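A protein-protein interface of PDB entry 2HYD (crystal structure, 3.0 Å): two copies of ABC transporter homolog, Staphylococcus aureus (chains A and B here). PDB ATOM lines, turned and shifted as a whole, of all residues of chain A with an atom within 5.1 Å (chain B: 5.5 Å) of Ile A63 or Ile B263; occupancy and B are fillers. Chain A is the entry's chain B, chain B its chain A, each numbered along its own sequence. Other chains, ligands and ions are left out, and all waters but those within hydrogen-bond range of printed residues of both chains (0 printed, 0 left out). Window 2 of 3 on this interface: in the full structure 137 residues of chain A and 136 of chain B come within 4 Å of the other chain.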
ATOM      1  N   LEU A  36     -22.441 -24.678  13.155  1.00  0.00           N
ATOM      2  CA  LEU A  36     -21.489 -25.654  13.670  1.00  0.00           C
ATOM      3  C   LEU A  36     -22.155 -26.657  14.629  1.00  0.00           C
ATOM      4  O   LEU A  36     -21.700 -27.791  14.757  1.00  0.00           O
ATOM      5  CB  LEU A  36     -20.347 -24.963  14.419  1.00  0.00           C
ATOM      6  CG  LEU A  36     -19.345 -25.975  14.989  1.00  0.00           C
ATOM      7  CD1 LEU A  36     -18.524 -26.559  13.846  1.00  0.00           C
ATOM      8  CD2 LEU A  36     -18.443 -25.314  16.015  1.00  0.00           C
ATOM      9  N   ILE A  37     -23.210 -26.260  15.334  1.00  0.00           N
ATOM     10  CA  ILE A  37     -23.871 -27.187  16.262  1.00  0.00           C
ATOM     11  C   ILE A  37     -24.503 -28.359  15.504  1.00  0.00           C
ATOM     12  O   ILE A  37     -24.540 -29.493  15.992  1.00  0.00           O
ATOM     13  CB  ILE A  37     -24.971 -26.473  17.070  1.00  0.00           C
ATOM     14  CG1 ILE A  37     -24.375 -25.259  17.787  1.00  0.00           C
ATOM     15  CG2 ILE A  37     -25.596 -27.441  18.073  1.00  0.00           C
ATOM     16  CD1 ILE A  37     -25.414 -24.328  18.382  1.00  0.00           C
ATOM     17  N   ALA A  40     -21.636 -31.349  14.036  1.00  0.00           N
ATOM     18  CA  ALA A  40     -21.193 -32.424  14.918  1.00  0.00           C
ATOM     19  C   ALA A  40     -22.377 -33.338  15.211  1.00  0.00           C
ATOM     20  O   ALA A  40     -22.273 -34.564  15.114  1.00  0.00           O
ATOM     21  CB  ALA A  40     -20.639 -31.855  16.213  1.00  0.00           C
ATOM     22  N   HIS A  58     -13.006 -35.598  11.329  1.00  0.00           N
ATOM     23  CA  HIS A  58     -13.793 -34.506  10.773  1.00  0.00           C
ATOM     24  C   HIS A  58     -14.074 -33.488  11.860  1.00  0.00           C
ATOM     25  O   HIS A  58     -14.278 -32.310  11.580  1.00  0.00           O
ATOM     26  CB  HIS A  58     -15.112 -35.023  10.206  1.00  0.00           C
ATOM     27  CG  HIS A  58     -14.944 -35.957   9.050  1.00  0.00           C
ATOM     28  ND1 HIS A  58     -14.020 -35.742   8.049  1.00  0.00           N
ATOM     29  CD2 HIS A  58     -15.600 -37.093   8.717  1.00  0.00           C
ATOM     30  CE1 HIS A  58     -14.114 -36.705   7.151  1.00  0.00           C
ATOM     31  NE2 HIS A  58     -15.066 -37.538   7.532  1.00  0.00           N
ATOM     32  N   LEU A  59     -14.090 -33.952  13.105  1.00  0.00           N
ATOM     33  CA  LEU A  59     -14.333 -33.069  14.234  1.00  0.00           C
ATOM     34  C   LEU A  59     -13.047 -32.339  14.599  1.00  0.00           C
ATOM     35  O   LEU A  59     -13.040 -31.498  15.492  1.00  0.00           O
ATOM     36  CB  LEU A  59     -14.812 -33.856  15.450  1.00  0.00           C
ATOM     37  CG  LEU A  59     -15.239 -32.952  16.606  1.00  0.00           C
ATOM     38  CD1 LEU A  59     -16.657 -32.465  16.344  1.00  0.00           C
ATOM     39  CD2 LEU A  59     -15.161 -33.700  17.927  1.00  0.00           C
ATOM     40  N   THR A  60     -11.959 -32.671  13.912  1.00  0.00           N
ATOM     41  CA  THR A  60     -10.669 -32.033  14.175  1.00  0.00           C
ATOM     42  C   THR A  60     -10.267 -31.105  13.023  1.00  0.00           C
ATOM     43  O   THR A  60      -9.145 -30.591  12.967  1.00  0.00           O
ATOM     44  CB  THR A  60      -9.577 -33.096  14.429  1.00  0.00           C
ATOM     45  OG1 THR A  60     -10.005 -33.946  15.503  1.00  0.00           O
ATOM     46  CG2 THR A  60      -8.241 -32.439  14.810  1.00  0.00           C
ATOM     47  N   ILE A  61     -11.206 -30.907  12.104  1.00  0.00           N
ATOM     48  CA  ILE A  61     -11.022 -30.015  10.965  1.00  0.00           C
ATOM     49  C   ILE A  61     -12.184 -29.025  11.068  1.00  0.00           C
ATOM     50  O   ILE A  61     -12.119 -27.902  10.565  1.00  0.00           O
ATOM     51  CB  ILE A  61     -11.100 -30.765   9.602  1.00  0.00           C
ATOM     52  CG1 ILE A  61     -12.499 -31.358   9.406  1.00  0.00           C
ATOM     53  CG2 ILE A  61     -10.031 -31.852   9.544  1.00  0.00           C
ATOM     54  CD1 ILE A  61     -12.785 -31.811   7.991  1.00  0.00           C
ATOM     55  N   ALA A  62     -13.248 -29.468  11.738  1.00  0.00           N
ATOM     56  CA  ALA A  62     -14.444 -28.659  11.961  1.00  0.00           C
ATOM     57  C   ALA A  62     -14.198 -27.834  13.223  1.00  0.00           C
ATOM     58  O   ALA A  62     -14.700 -26.712  13.362  1.00  0.00           O
ATOM     59  CB  ALA A  62     -15.661 -29.556  12.140  1.00  0.00           C
ATOM     60  N   ILE A  63     -13.445 -28.418  14.155  1.00  0.00           N
ATOM     61  CA  ILE A  63     -13.068 -27.720  15.378  1.00  0.00           C
ATOM     62  C   ILE A  63     -11.736 -27.114  14.970  1.00  0.00           C
ATOM     63  O   ILE A  63     -11.017 -26.502  15.762  1.00  0.00           O
ATOM     64  CB  ILE A  63     -12.895 -28.680  16.590  1.00  0.00           C
ATOM     65  CG1 ILE A  63     -14.271 -29.124  17.097  1.00  0.00           C
ATOM     66  CG2 ILE A  63     -12.149 -27.982  17.732  1.00  0.00           C
ATOM     67  CD1 ILE A  63     -15.150 -27.985  17.585  1.00  0.00           C
ATOM     68  N   GLY A  64     -11.409 -27.303  13.699  1.00  0.00           N
ATOM     69  CA  GLY A  64     -10.182 -26.729  13.196  1.00  0.00           C
ATOM     70  C   GLY A  64     -10.546 -25.503  12.382  1.00  0.00           C
ATOM     71  O   GLY A  64      -9.882 -24.465  12.461  1.00  0.00           O
ATOM     72  N   ILE A  65     -11.616 -25.640  11.598  1.00  0.00           N
ATOM     73  CA  ILE A  65     -12.122 -24.567  10.753  1.00  0.00           C
ATOM     74  C   ILE A  65     -12.680 -23.425  11.600  1.00  0.00           C
ATOM     75  O   ILE A  65     -12.377 -22.253  11.358  1.00  0.00           O
ATOM     76  CB  ILE A  65     -13.249 -25.086   9.801  1.00  0.00           C
ATOM     77  CG1 ILE A  65     -12.776 -24.983   8.354  1.00  0.00           C
ATOM     78  CG2 ILE A  65     -14.559 -24.289  10.013  1.00  0.00           C
ATOM     79  CD1 ILE A  65     -13.848 -25.295   7.319  1.00  0.00           C
ATOM     80  N   ALA A  66     -13.499 -23.778  12.590  1.00  0.00           N
ATOM     81  CA  ALA A  66     -14.116 -22.792  13.475  1.00  0.00           C
ATOM     82  C   ALA A  66     -13.061 -21.907  14.117  1.00  0.00           C
ATOM     83  O   ALA A  66     -13.127 -20.677  14.025  1.00  0.00           O
ATOM     84  CB  ALA A  66     -14.931 -23.498  14.554  1.00  0.00           C
ATOM     85  N   LEU A  67     -12.086 -22.541  14.762  1.00  0.00           N
ATOM     86  CA  LEU A  67     -11.018 -21.806  15.415  1.00  0.00           C
ATOM     87  C   LEU A  67     -10.354 -20.833  14.460  1.00  0.00           C
ATOM     88  O   LEU A  67     -10.157 -19.669  14.797  1.00  0.00           O
ATOM     89  CB  LEU A  67      -9.982 -22.769  15.985  1.00  0.00           C
ATOM     90  CG  LEU A  67     -10.516 -23.625  17.137  1.00  0.00           C
ATOM     91  CD1 LEU A  67      -9.362 -24.392  17.756  1.00  0.00           C
ATOM     92  CD2 LEU A  67     -11.182 -22.738  18.180  1.00  0.00           C
ATOM     93  N   GLY B 258     -14.960 -19.632  23.408  1.00  0.00           N
ATOM     94  CA  GLY B 258     -15.879 -20.198  24.376  1.00  0.00           C
ATOM     95  C   GLY B 258     -16.833 -21.246  23.839  1.00  0.00           C
ATOM     96  O   GLY B 258     -16.715 -22.409  24.211  1.00  0.00           O
ATOM     97  N   PRO B 259     -17.805 -20.875  22.988  1.00  0.00           N
ATOM     98  CA  PRO B 259     -18.736 -21.874  22.453  1.00  0.00           C
ATOM     99  C   PRO B 259     -18.009 -22.988  21.700  1.00  0.00           C
ATOM    100  O   PRO B 259     -18.481 -24.128  21.661  1.00  0.00           O
ATOM    101  CB  PRO B 259     -19.636 -21.051  21.539  1.00  0.00           C
ATOM    102  CG  PRO B 259     -19.691 -19.736  22.245  1.00  0.00           C
ATOM    103  CD  PRO B 259     -18.242 -19.515  22.632  1.00  0.00           C
ATOM    104  N   ILE B 260     -16.864 -22.659  21.103  1.00  0.00           N
ATOM    105  CA  ILE B 260     -16.091 -23.663  20.372  1.00  0.00           C
ATOM    106  C   ILE B 260     -15.558 -24.750  21.306  1.00  0.00           C
ATOM    107  O   ILE B 260     -15.972 -25.910  21.218  1.00  0.00           O
ATOM    108  CB  ILE B 260     -14.899 -23.032  19.600  1.00  0.00           C
ATOM    109  CG1 ILE B 260     -15.407 -22.411  18.295  1.00  0.00           C
ATOM    110  CG2 ILE B 260     -13.830 -24.092  19.305  1.00  0.00           C
ATOM    111  CD1 ILE B 260     -14.305 -21.925  17.374  1.00  0.00           C
ATOM    112  N   ILE B 261     -14.651 -24.381  22.205  1.00  0.00           N
ATOM    113  CA  ILE B 261     -14.089 -25.355  23.125  1.00  0.00           C
ATOM    114  C   ILE B 261     -15.160 -26.167  23.867  1.00  0.00           C
ATOM    115  O   ILE B 261     -14.859 -27.170  24.504  1.00  0.00           O
ATOM    116  CB  ILE B 261     -13.134 -24.685  24.140  1.00  0.00           C
ATOM    117  CG1 ILE B 261     -12.461 -25.762  24.991  1.00  0.00           C
ATOM    118  CG2 ILE B 261     -13.892 -23.688  25.008  1.00  0.00           C
ATOM    119  CD1 ILE B 261     -11.281 -25.269  25.765  1.00  0.00           C
ATOM    120  N   VAL B 262     -16.410 -25.749  23.829  1.00  0.00           N
ATOM    121  CA  VAL B 262     -17.393 -26.578  24.491  1.00  0.00           C
ATOM    122  C   VAL B 262     -17.680 -27.672  23.473  1.00  0.00           C
ATOM    123  O   VAL B 262     -17.724 -28.850  23.815  1.00  0.00           O
ATOM    124  CB  VAL B 262     -18.660 -25.786  24.850  1.00  0.00           C
ATOM    125  CG1 VAL B 262     -19.807 -26.737  25.194  1.00  0.00           C
ATOM    126  CG2 VAL B 262     -18.361 -24.896  26.053  1.00  0.00           C
ATOM    127  N   ILE B 263     -17.826 -27.272  22.211  1.00  0.00           N
ATOM    128  CA  ILE B 263     -18.086 -28.212  21.125  1.00  0.00           C
ATOM    129  C   ILE B 263     -16.876 -29.108  20.837  1.00  0.00           C
ATOM    130  O   ILE B 263     -17.036 -30.288  20.523  1.00  0.00           O
ATOM    131  CB  ILE B 263     -18.503 -27.469  19.814  1.00  0.00           C
ATOM    132  CG1 ILE B 263     -19.988 -27.084  19.885  1.00  0.00           C
ATOM    133  CG2 ILE B 263     -18.222 -28.343  18.592  1.00  0.00           C
ATOM    134  CD1 ILE B 263     -20.568 -26.535  18.579  1.00  0.00           C
ATOM    135  N   GLY B 264     -15.672 -28.553  20.945  1.00  0.00           N
ATOM    136  CA  GLY B 264     -14.478 -29.344  20.695  1.00  0.00           C
ATOM    137  C   GLY B 264     -14.356 -30.535  21.634  1.00  0.00           C
ATOM    138  O   GLY B 264     -14.082 -31.658  21.205  1.00  0.00           O
ATOM    139  N   VAL B 265     -14.556 -30.286  22.923  1.00  0.00           N
ATOM    140  CA  VAL B 265     -14.476 -31.337  23.927  1.00  0.00           C
ATOM    141  C   VAL B 265     -15.805 -32.073  24.015  1.00  0.00           C
ATOM    142  O   VAL B 265     -15.862 -33.293  23.873  1.00  0.00           O
ATOM    143  CB  VAL B 265     -14.135 -30.758  25.325  1.00  0.00           C
ATOM    144  CG1 VAL B 265     -14.298 -31.838  26.401  1.00  0.00           C
ATOM    145  CG2 VAL B 265     -12.704 -30.203  25.328  1.00  0.00           C
ATOM    146  N   GLY B 266     -16.871 -31.315  24.247  1.00  0.00           N
ATOM    147  CA  GLY B 266     -18.196 -31.900  24.359  1.00  0.00           C
ATOM    148  C   GLY B 266     -18.493 -32.975  23.330  1.00  0.00           C
ATOM    149  O   GLY B 266     -19.061 -34.017  23.659  1.00  0.00           O
ATOM    150  N   ALA B 267     -18.113 -32.724  22.083  1.00  0.00           N
ATOM    151  CA  ALA B 267     -18.346 -33.688  21.017  1.00  0.00           C
ATOM    152  C   ALA B 267     -17.463 -34.909  21.224  1.00  0.00           C
ATOM    153  O   ALA B 267     -17.921 -36.046  21.093  1.00  0.00           O
ATOM    154  CB  ALA B 267     -18.058 -33.057  19.672  1.00  0.00           C
ATOM    155  N   TYR B 268     -16.193 -34.667  21.545  1.00  0.00           N
ATOM    156  CA  TYR B 268     -15.256 -35.759  21.779  1.00  0.00           C
ATOM    157  C   TYR B 268     -15.724 -36.607  22.957  1.00  0.00           C
ATOM    158  O   TYR B 268     -15.607 -37.830  22.934  1.00  0.00           O
ATOM    159  CB  TYR B 268     -13.850 -35.232  22.074  1.00  0.00           C
ATOM    160  CG  TYR B 268     -12.858 -36.344  22.327  1.00  0.00           C
ATOM    161  CD1 TYR B 268     -12.459 -37.194  21.294  1.00  0.00           C
ATOM    162  CD2 TYR B 268     -12.354 -36.581  23.608  1.00  0.00           C
ATOM    163  CE1 TYR B 268     -11.585 -38.254  21.529  1.00  0.00           C
ATOM    164  CE2 TYR B 268     -11.480 -37.640  23.854  1.00  0.00           C
ATOM    165  CZ  TYR B 268     -11.101 -38.472  22.811  1.00  0.00           C
ATOM    166  OH  TYR B 268     -10.245 -39.523  23.051  1.00  0.00           O
ATOM    167  N   VAL B 284     -25.901 -27.055  24.581  1.00  0.00           N
ATOM    168  CA  VAL B 284     -25.528 -26.135  23.517  1.00  0.00           C
ATOM    169  C   VAL B 284     -26.586 -25.093  23.148  1.00  0.00           C
ATOM    170  O   VAL B 284     -26.282 -24.096  22.487  1.00  0.00           O
ATOM    171  CB  VAL B 284     -25.098 -26.946  22.271  1.00  0.00           C
ATOM    172  CG1 VAL B 284     -25.161 -26.090  21.019  1.00  0.00           C
ATOM    173  CG2 VAL B 284     -23.672 -27.467  22.483  1.00  0.00           C
ATOM    174  N   LEU B 287     -25.855 -21.945  25.167  1.00  0.00           N
ATOM    175  CA  LEU B 287     -24.595 -21.261  24.854  1.00  0.00           C
ATOM    176  C   LEU B 287     -24.760 -19.748  24.693  1.00  0.00           C
ATOM    177  O   LEU B 287     -23.865 -18.969  25.032  1.00  0.00           O
ATOM    178  CB  LEU B 287     -23.983 -21.832  23.573  1.00  0.00           C
ATOM    179  CG  LEU B 287     -23.295 -23.191  23.681  1.00  0.00           C
ATOM    180  CD1 LEU B 287     -22.790 -23.609  22.309  1.00  0.00           C
ATOM    181  CD2 LEU B 287     -22.145 -23.107  24.676  1.00  0.00           C
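Among the printed residues, pairs that only touch across the chains: Leu A67 with Ile B260 (3.2 Å), Ile A37 with Val B284 (3.2 Å), Ile A63 with Ile B263 (3.3 Å), Ala A66 with Ile B260 (3.3 Å), Leu A59 with Ala B267 (3.4 Å), Ile A63 with Gly B264 (3.4 Å), Leu A36 with Ile B263 (3.5 Å) and Leu A59 with Tyr B268 (3.9 Å).
Of the printed residues of chain B, Ile A37 touches Val B284. Ala A40 touches none of the printed residues of chain B. Of the printed residues of chain B, Leu A59 touches Ala B267 (3.4 Å) and Tyr B268 (3.9 Å). Of chain B, only Ile B263 and Gly B264 come within 4 Å of Ile A63. Gly B258 touches none of the printed residues of chain A. Of chain A, only Leu A36 and Ile A63 come within 4 Å of Ile B263. Of the printed residues of chain A, Gly B264 touches Ile A63 (3.4 Å). Of the printed residues of chain A, Tyr B268 touches Leu A59 (3.9 Å). The nearest residue of chain B that does not touch Ile A63 is Ile B260 (4.3 Å). The nearest residue of chain A that does not touch Ile B263 is Ile A37 (4.1 Å).
Of the 13 printed residues of chain A, 6 touch a printed residue of chain B. Hydrophobic or aromatic side chains of chain A that line the printed part of chain B: Leu A36, Ile A37, Leu A59, Ile A63, Ala A66 and Leu A67. Printed residues of chain B that touch a printed residue of chain A: Ile B260, Ile B263, Gly B264, Ala B267, Tyr B268 and Val B284. Along chain B the printed residues that touch a printed residue of chain A span positions 260 to 284.
No position is printed for both chains. Of the 8 pairs that touch across the chains among the printed residues, none has its exchanged pair printed and touching as well.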
